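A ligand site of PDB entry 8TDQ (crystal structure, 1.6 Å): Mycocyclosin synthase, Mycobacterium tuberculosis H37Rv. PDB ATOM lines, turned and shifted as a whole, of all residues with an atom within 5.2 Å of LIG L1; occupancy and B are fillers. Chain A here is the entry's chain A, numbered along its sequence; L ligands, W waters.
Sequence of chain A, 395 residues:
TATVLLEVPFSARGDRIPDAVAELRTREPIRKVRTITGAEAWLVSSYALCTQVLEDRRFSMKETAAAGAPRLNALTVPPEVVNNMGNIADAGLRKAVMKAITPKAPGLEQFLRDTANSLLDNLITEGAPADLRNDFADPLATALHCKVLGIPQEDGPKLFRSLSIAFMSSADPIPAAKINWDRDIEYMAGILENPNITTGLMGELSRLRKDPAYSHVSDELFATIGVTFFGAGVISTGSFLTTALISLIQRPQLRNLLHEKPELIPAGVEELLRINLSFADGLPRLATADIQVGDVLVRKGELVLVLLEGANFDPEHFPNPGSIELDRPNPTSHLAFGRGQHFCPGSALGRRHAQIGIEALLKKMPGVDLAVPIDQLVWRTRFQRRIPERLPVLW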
ATOM      1  N   MET A  61      11.679 -36.370 -13.673  1.00  0.00           N
ATOM      2  CA  MET A  61      11.135 -35.054 -14.028  1.00  0.00           C
ATOM      3  C   MET A  61      11.448 -34.011 -12.954  1.00  0.00           C
ATOM      4  O   MET A  61      11.850 -32.890 -13.279  1.00  0.00           O
ATOM      5  CB  MET A  61       9.641 -35.176 -14.383  1.00  0.00           C
ATOM      6  CG  MET A  61       8.846 -33.843 -14.479  1.00  0.00           C
ATOM      7  SD  MET A  61       7.116 -33.892 -13.923  1.00  0.00           S
ATOM      8  CE  MET A  61       6.469 -34.660 -15.408  1.00  0.00           C
ATOM      9  N   THR A  76       8.778 -21.339 -15.552  1.00  0.00           N
ATOM     10  CA  THR A  76       7.772 -20.298 -15.369  1.00  0.00           C
ATOM     11  C   THR A  76       6.985 -20.509 -14.083  1.00  0.00           C
ATOM     12  O   THR A  76       6.042 -19.752 -13.820  1.00  0.00           O
ATOM     13  CB  THR A  76       6.804 -20.244 -16.555  1.00  0.00           C
ATOM     14  OG1 THR A  76       6.053 -21.455 -16.637  1.00  0.00           O
ATOM     15  CG2 THR A  76       7.563 -20.062 -17.877  1.00  0.00           C
ATOM     16  N   VAL A  77       7.366 -21.495 -13.271  1.00  0.00           N
ATOM     17  CA  VAL A  77       6.736 -21.801 -11.997  1.00  0.00           C
ATOM     18  C   VAL A  77       7.835 -21.943 -10.957  1.00  0.00           C
ATOM     19  O   VAL A  77       9.012 -22.127 -11.295  1.00  0.00           O
ATOM     20  CB  VAL A  77       5.886 -23.105 -12.081  1.00  0.00           C
ATOM     21  CG1 VAL A  77       4.769 -22.925 -13.118  1.00  0.00           C
ATOM     22  CG2 VAL A  77       6.760 -24.288 -12.447  1.00  0.00           C
ATOM     23  N   VAL A  81       7.173 -26.700  -7.845  1.00  0.00           N
ATOM     24  CA  VAL A  81       5.967 -27.079  -8.583  1.00  0.00           C
ATOM     25  C   VAL A  81       6.261 -28.038  -9.733  1.00  0.00           C
ATOM     26  O   VAL A  81       5.332 -28.673 -10.253  1.00  0.00           O
ATOM     27  CB  VAL A  81       5.258 -25.791  -9.053  1.00  0.00           C
ATOM     28  CG1 VAL A  81       4.039 -26.069  -9.936  1.00  0.00           C
ATOM     29  CG2 VAL A  81       4.857 -24.950  -7.837  1.00  0.00           C
ATOM     30  N   VAL A  82       7.522 -28.178 -10.149  1.00  0.00           N
ATOM     31  CA  VAL A  82       7.853 -29.232 -11.108  1.00  0.00           C
ATOM     32  C   VAL A  82       7.505 -30.600 -10.524  1.00  0.00           C
ATOM     33  O   VAL A  82       7.111 -31.517 -11.246  1.00  0.00           O
ATOM     34  CB  VAL A  82       9.341 -29.136 -11.506  1.00  0.00           C
ATOM     35  CG1 VAL A  82       9.736 -30.297 -12.423  1.00  0.00           C
ATOM     36  CG2 VAL A  82       9.610 -27.785 -12.167  1.00  0.00           C
ATOM     37  N   ASN A  84       4.871 -31.267  -8.838  1.00  0.00           N
ATOM     38  CA  ASN A  84       3.495 -31.016  -8.404  1.00  0.00           C
ATOM     39  C   ASN A  84       2.778 -32.305  -7.988  1.00  0.00           C
ATOM     40  O   ASN A  84       2.272 -32.402  -6.864  1.00  0.00           O
ATOM     41  CB  ASN A  84       2.741 -30.331  -9.545  1.00  0.00           C
ATOM     42  CG  ASN A  84       1.411 -29.730  -9.099  1.00  0.00           C
ATOM     43  OD1 ASN A  84       1.273 -29.209  -7.983  1.00  0.00           O
ATOM     44  ND2 ASN A  84       0.433 -29.757 -10.001  1.00  0.00           N
ATOM     45  N   ALA A 166       2.365 -18.058 -19.211  1.00  0.00           N
ATOM     46  CA  ALA A 166       2.696 -19.164 -18.328  1.00  0.00           C
ATOM     47  C   ALA A 166       3.271 -20.345 -19.088  1.00  0.00           C
ATOM     48  O   ALA A 166       4.125 -21.084 -18.577  1.00  0.00           O
ATOM     49  CB  ALA A 166       1.440 -19.608 -17.560  1.00  0.00           C
ATOM     50  N   PHE A 167       2.778 -20.592 -20.305  1.00  0.00           N
ATOM     51  CA  PHE A 167       3.221 -21.745 -21.064  1.00  0.00           C
ATOM     52  C   PHE A 167       4.173 -21.359 -22.188  1.00  0.00           C
ATOM     53  O   PHE A 167       4.384 -22.145 -23.113  1.00  0.00           O
ATOM     54  CB  PHE A 167       2.000 -22.532 -21.547  1.00  0.00           C
ATOM     55  CG  PHE A 167       1.437 -23.378 -20.461  1.00  0.00           C
ATOM     56  CD1 PHE A 167       1.994 -24.602 -20.198  1.00  0.00           C
ATOM     57  CD2 PHE A 167       0.464 -22.890 -19.610  1.00  0.00           C
ATOM     58  CE1 PHE A 167       1.529 -25.383 -19.137  1.00  0.00           C
ATOM     59  CE2 PHE A 167      -0.017 -23.668 -18.552  1.00  0.00           C
ATOM     60  CZ  PHE A 167       0.521 -24.909 -18.306  1.00  0.00           C
ATOM     61  N   TRP A 181       1.561 -15.491 -11.767  1.00  0.00           N
ATOM     62  CA  TRP A 181       1.513 -16.621 -10.828  1.00  0.00           C
ATOM     63  C   TRP A 181       1.077 -16.164  -9.434  1.00  0.00           C
ATOM     64  O   TRP A 181       0.163 -16.747  -8.842  1.00  0.00           O
ATOM     65  CB  TRP A 181       2.892 -17.296 -10.761  1.00  0.00           C
ATOM     66  CG  TRP A 181       2.950 -18.454  -9.777  1.00  0.00           C
ATOM     67  CD1 TRP A 181       3.409 -18.409  -8.487  1.00  0.00           C
ATOM     68  CD2 TRP A 181       2.527 -19.796 -10.016  1.00  0.00           C
ATOM     69  NE1 TRP A 181       3.308 -19.657  -7.913  1.00  0.00           N
ATOM     70  CE2 TRP A 181       2.768 -20.527  -8.826  1.00  0.00           C
ATOM     71  CE3 TRP A 181       2.002 -20.473 -11.119  1.00  0.00           C
ATOM     72  CZ2 TRP A 181       2.477 -21.879  -8.704  1.00  0.00           C
ATOM     73  CZ3 TRP A 181       1.709 -21.838 -10.998  1.00  0.00           C
ATOM     74  CH2 TRP A 181       1.939 -22.518  -9.794  1.00  0.00           C
ATOM     75  N   VAL A 227      -4.389 -23.654  -9.335  1.00  0.00           N
ATOM     76  CA  VAL A 227      -3.766 -22.916 -10.434  1.00  0.00           C
ATOM     77  C   VAL A 227      -3.185 -23.865 -11.474  1.00  0.00           C
ATOM     78  O   VAL A 227      -3.339 -23.643 -12.676  1.00  0.00           O
ATOM     79  CB  VAL A 227      -2.677 -21.955  -9.905  1.00  0.00           C
ATOM     80  CG1 VAL A 227      -1.968 -21.268 -11.076  1.00  0.00           C
ATOM     81  CG2 VAL A 227      -3.284 -20.901  -8.959  1.00  0.00           C
ATOM     82  N   THR A 228      -2.494 -24.912 -11.012  1.00  0.00           N
ATOM     83  CA  THR A 228      -1.796 -25.787 -11.961  1.00  0.00           C
ATOM     84  C   THR A 228      -2.779 -26.642 -12.749  1.00  0.00           C
ATOM     85  O   THR A 228      -2.595 -26.868 -13.951  1.00  0.00           O
ATOM     86  CB  THR A 228      -0.783 -26.692 -11.239  1.00  0.00           C
ATOM     87  OG1 THR A 228      -1.427 -27.455 -10.223  1.00  0.00           O
ATOM     88  CG2 THR A 228       0.300 -25.840 -10.601  1.00  0.00           C
ATOM     89  N   GLY A 231      -4.461 -24.400 -15.321  1.00  0.00           N
ATOM     90  CA  GLY A 231      -3.538 -24.042 -16.402  1.00  0.00           C
ATOM     91  C   GLY A 231      -3.188 -25.210 -17.311  1.00  0.00           C
ATOM     92  O   GLY A 231      -3.314 -25.127 -18.537  1.00  0.00           O
ATOM     93  N   ALA A 232      -2.715 -26.319 -16.732  1.00  0.00           N
ATOM     94  CA  ALA A 232      -2.357 -27.452 -17.571  1.00  0.00           C
ATOM     95  C   ALA A 232      -3.583 -28.014 -18.306  1.00  0.00           C
ATOM     96  O   ALA A 232      -3.494 -28.415 -19.468  1.00  0.00           O
ATOM     97  CB  ALA A 232      -1.689 -28.542 -16.734  1.00  0.00           C
ATOM     98  N   SER A 236      -3.933 -27.637 -22.417  1.00  0.00           N
ATOM     99  CA  SER A 236      -3.770 -28.919 -23.085  1.00  0.00           C
ATOM    100  C   SER A 236      -5.013 -29.294 -23.883  1.00  0.00           C
ATOM    101  O   SER A 236      -4.917 -29.718 -25.041  1.00  0.00           O
ATOM    102  CB  SER A 236      -3.453 -30.014 -22.059  1.00  0.00           C
ATOM    103  OG  SER A 236      -2.233 -29.734 -21.367  1.00  0.00           O
ATOM    104  N   PHE A 279       2.173 -30.821 -28.554  1.00  0.00           N
ATOM    105  CA  PHE A 279       3.320 -30.554 -27.671  1.00  0.00           C
ATOM    106  C   PHE A 279       4.481 -30.051 -28.530  1.00  0.00           C
ATOM    107  O   PHE A 279       4.880 -30.705 -29.490  1.00  0.00           O
ATOM    108  CB  PHE A 279       3.718 -31.812 -26.890  1.00  0.00           C
ATOM    109  CG  PHE A 279       3.040 -31.923 -25.550  1.00  0.00           C
ATOM    110  CD1 PHE A 279       1.686 -32.177 -25.467  1.00  0.00           C
ATOM    111  CD2 PHE A 279       3.777 -31.769 -24.365  1.00  0.00           C
ATOM    112  CE1 PHE A 279       1.054 -32.287 -24.227  1.00  0.00           C
ATOM    113  CE2 PHE A 279       3.139 -31.870 -23.121  1.00  0.00           C
ATOM    114  CZ  PHE A 279       1.782 -32.129 -23.060  1.00  0.00           C
ATOM    115  N   GLN A 384       4.974 -23.726 -25.326  1.00  0.00           N
ATOM    116  CA  GLN A 384       5.013 -25.147 -25.004  1.00  0.00           C
ATOM    117  C   GLN A 384       3.987 -25.960 -25.775  1.00  0.00           C
ATOM    118  O   GLN A 384       4.027 -27.206 -25.728  1.00  0.00           O
ATOM    119  CB  GLN A 384       4.814 -25.355 -23.495  1.00  0.00           C
ATOM    120  CG  GLN A 384       6.020 -24.832 -22.678  1.00  0.00           C
ATOM    121  CD  GLN A 384       5.839 -24.991 -21.192  1.00  0.00           C
ATOM    122  OE1 GLN A 384       5.331 -26.008 -20.721  1.00  0.00           O
ATOM    123  NE2 GLN A 384       6.289 -23.979 -20.425  1.00  0.00           N
ATOM    124  N   ARG A 385       3.054 -25.309 -26.454  1.00  0.00           N
ATOM    125  CA  ARG A 385       2.114 -25.967 -27.343  1.00  0.00           C
ATOM    126  C   ARG A 385       2.217 -25.339 -28.726  1.00  0.00           C
ATOM    127  O   ARG A 385       2.609 -24.174 -28.859  1.00  0.00           O
ATOM    128  CB  ARG A 385       0.660 -25.840 -26.847  1.00  0.00           C
ATOM    129  CG  ARG A 385       0.365 -26.514 -25.502  1.00  0.00           C
ATOM    130  CD  ARG A 385       0.509 -28.025 -25.571  1.00  0.00           C
ATOM    131  NE  ARG A 385       0.178 -28.616 -24.285  1.00  0.00           N
ATOM    132  CZ  ARG A 385       1.034 -28.688 -23.273  1.00  0.00           C
ATOM    133  NH1 ARG A 385       2.283 -28.242 -23.386  1.00  0.00           N
ATOM    134  NH2 ARG A 385       0.631 -29.235 -22.125  1.00  0.00           N
HETATM  135  O1  LIG L   1       6.273 -28.197 -13.870  1.00  0.00           O
HETATM  136  C1  LIG L   1       5.142 -28.633 -13.744  1.00  0.00           C
HETATM  137  C2  LIG L   1       4.884 -30.137 -13.663  1.00  0.00           C
HETATM  138  C3  LIG L   1       5.295 -30.864 -14.966  1.00  0.00           C
HETATM  139  C4  LIG L   1       4.489 -30.461 -16.161  1.00  0.00           C
HETATM  140  C5  LIG L   1       4.899 -29.411 -16.995  1.00  0.00           C
HETATM  141  C6  LIG L   1       4.171 -29.035 -18.109  1.00  0.00           C
HETATM  142  C7  LIG L   1       2.991 -29.705 -18.424  1.00  0.00           C
HETATM  143  O2  LIG L   1       2.304 -29.302 -19.509  1.00  0.00           O
HETATM  144  C8  LIG L   1       2.571 -30.773 -17.622  1.00  0.00           C
HETATM  145  C9  LIG L   1       3.322 -31.130 -16.516  1.00  0.00           C
HETATM  146  N1  LIG L   1       3.535 -30.465 -13.235  1.00  0.00           N
HETATM  147  N2  LIG L   1       4.088 -27.815 -13.653  1.00  0.00           N
HETATM  148  C10 LIG L   1       2.704 -28.182 -13.541  1.00  0.00           C
HETATM  149  C11 LIG L   1       2.484 -29.633 -13.144  1.00  0.00           C
HETATM  150  O3  LIG L   1       1.380 -29.972 -12.780  1.00  0.00           O
HETATM  151  C12 LIG L   1       1.972 -27.857 -14.874  1.00  0.00           C
HETATM  152  C13 LIG L   1       1.896 -26.353 -15.019  1.00  0.00           C
HETATM  153  C14 LIG L   1       2.924 -25.609 -15.595  1.00  0.00           C
HETATM  154  C15 LIG L   1       2.865 -24.225 -15.711  1.00  0.00           C
HETATM  155  C16 LIG L   1       1.747 -23.547 -15.208  1.00  0.00           C
HETATM  156  O4  LIG L   1       1.599 -22.211 -15.267  1.00  0.00           O
HETATM  157  C17 LIG L   1       0.696 -24.279 -14.631  1.00  0.00           C
HETATM  158  C18 LIG L   1       0.780 -25.658 -14.548  1.00  0.00           C
HETATM  159  C1  LG2 L   2       0.769 -34.596 -17.657  1.00  0.00           C
HETATM  160  C2  LG2 L   2      -0.915 -34.458 -22.219  1.00  0.00           C
HETATM  161  C3  LG2 L   2      -5.211 -32.920 -20.497  1.00  0.00           C
HETATM  162  C4  LG2 L   2      -3.169 -32.187 -16.178  1.00  0.00           C
HETATM  163  C5  LG2 L   2       0.664 -34.755 -19.023  1.00  0.00           C
HETATM  164  C6  LG2 L   2       1.666 -35.362 -19.885  1.00  0.00           C
HETATM  165  C7  LG2 L   2       1.177 -35.312 -21.145  1.00  0.00           C
HETATM  166  C8  LG2 L   2      -0.118 -34.680 -21.114  1.00  0.00           C
HETATM  167  C9  LG2 L   2       1.871 -35.819 -22.424  1.00  0.00           C
HETATM  168  C10 LG2 L   2       3.025 -35.961 -19.414  1.00  0.00           C
HETATM  169  C11 LG2 L   2       4.082 -34.882 -19.197  1.00  0.00           C
HETATM  170  C12 LG2 L   2       5.417 -35.508 -18.865  1.00  0.00           C
HETATM  171  O1  LG2 L   2       5.494 -36.752 -18.667  1.00  0.00           O
HETATM  172  O2  LG2 L   2       6.423 -34.744 -18.821  1.00  0.00           O
HETATM  173  C13 LG2 L   2      -2.236 -34.034 -22.143  1.00  0.00           C
HETATM  174  C14 LG2 L   2      -3.153 -33.930 -23.255  1.00  0.00           C
HETATM  175  C15 LG2 L   2      -4.330 -33.478 -22.772  1.00  0.00           C
HETATM  176  C16 LG2 L   2      -4.200 -33.321 -21.340  1.00  0.00           C
HETATM  177  C17 LG2 L   2      -2.751 -34.261 -24.714  1.00  0.00           C
HETATM  178  C18 LG2 L   2      -5.668 -33.204 -23.508  1.00  0.00           C
HETATM  179  C19 LG2 L   2      -5.968 -33.773 -24.679  1.00  0.00           C
HETATM  180  C20 LG2 L   2      -5.057 -32.637 -19.156  1.00  0.00           C
HETATM  181  C21 LG2 L   2      -6.102 -32.200 -18.246  1.00  0.00           C
HETATM  182  C22 LG2 L   2      -5.535 -32.013 -17.042  1.00  0.00           C
HETATM  183  C23 LG2 L   2      -4.115 -32.289 -17.175  1.00  0.00           C
HETATM  184  C24 LG2 L   2      -7.591 -32.063 -18.696  1.00  0.00           C
HETATM  185  C25 LG2 L   2      -6.151 -31.558 -15.706  1.00  0.00           C
HETATM  186  C26 LG2 L   2      -7.413 -31.140 -15.592  1.00  0.00           C
HETATM  187  C27 LG2 L   2      -1.914 -32.764 -16.192  1.00  0.00           C
HETATM  188  C28 LG2 L   2      -0.970 -32.822 -15.085  1.00  0.00           C
HETATM  189  C29 LG2 L   2       0.117 -33.489 -15.492  1.00  0.00           C
HETATM  190  C30 LG2 L   2      -0.101 -33.873 -16.874  1.00  0.00           C
HETATM  191  C31 LG2 L   2      -1.215 -32.193 -13.698  1.00  0.00           C
HETATM  192  C32 LG2 L   2       1.395 -33.813 -14.657  1.00  0.00           C
HETATM  193  C33 LG2 L   2       1.336 -35.299 -14.231  1.00  0.00           C
HETATM  194  C34 LG2 L   2       2.545 -35.746 -13.427  1.00  0.00           C
HETATM  195  O3  LG2 L   2       2.497 -36.872 -12.870  1.00  0.00           O
HETATM  196  O4  LG2 L   2       3.542 -35.001 -13.304  1.00  0.00           O
HETATM  197  N1  LG2 L   2      -0.408 -34.346 -19.798  1.00  0.00           N
HETATM  198  N2  LG2 L   2      -2.899 -33.649 -20.999  1.00  0.00           N
HETATM  199  N3  LG2 L   2      -3.862 -32.683 -18.471  1.00  0.00           N
HETATM  200  N4  LG2 L   2      -1.342 -33.414 -17.268  1.00  0.00           N
HETATM  201 FE1  LG2 L   2      -2.217 -33.714 -19.094  1.00  0.00          FE
HETATM  202  O   HOH W   1      -0.480 -20.913 -14.538  1.00  0.00           O
HETATM  203  O   HOH W   2       4.324 -28.362 -21.326  1.00  0.00           O
HETATM  204  O   HOH W   3       7.164 -26.401 -15.722  1.00  0.00           O
HETATM  205  O   HOH W   4       3.931 -33.132 -11.549  1.00  0.00           O
HETATM  206  O   HOH W   5       3.425 -19.788 -14.787  1.00  0.00           O
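The guanidinium group of Arg 385 lies within hydrogen-bond range of an oxygen (O2) of LIG L1.
An oxygen (O3) of LIG L1 is in hydrogen-bond range of the side-chain amide nitrogen (ND2) of Asn 84 (2.9 Å).
OG of Ser 236 is in hydrogen-bond range of NH2 of Arg 385 (3.0 Å).
The backbone carbonyl oxygen (O) of Phe 167 lies within hydrogen-bond range of the backbone NH (N) of Gln 384, 2.8 Å away.
The backbone carbonyl oxygen of Ala 166 lies within hydrogen-bond range of the side-chain hydroxyl of Thr 76, 2.8 Å away.
The side-chain hydroxyl (OG1) of Thr 228 lies within hydrogen-bond range of the side-chain amide nitrogen (ND2) of Asn 84 (3.0 Å).
SD of Met 61 touches C3 of LIG L1, at 3.7 Å.
Val 77 touches LIG L1.
O of Val 81 touches C1 of LIG L1 (3.5 Å).
Val 82 touches LIG L1 (CA to O1, 3.3 Å).
CB of Ala 166 touches O4 of LIG L1 (3.5 Å).
Phe 167 touches LIG L1.
O of Thr 228 touches C18 of LIG L1, 3.6 Å away.
Hydrophobic or aromatic side chains that line LIG L1: Met 61, Val 77, Val 82, Ala 166 and Phe 167.
Water W2 lies within hydrogen-bond range of the side-chain amide oxygen of Gln 384 (2.6 Å), an oxygen (O2) of LIG L1 (2.9 Å) and the guanidinium group of Arg 385 (2.9 Å).
Water W5 bridges O of Thr 76 (2.8 Å) and O4 of LIG L1 (3.1 Å).
Water W4 lies within hydrogen-bond range of O4 of LG2 L2, N1 of LIG L1 and N of Asn 84.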
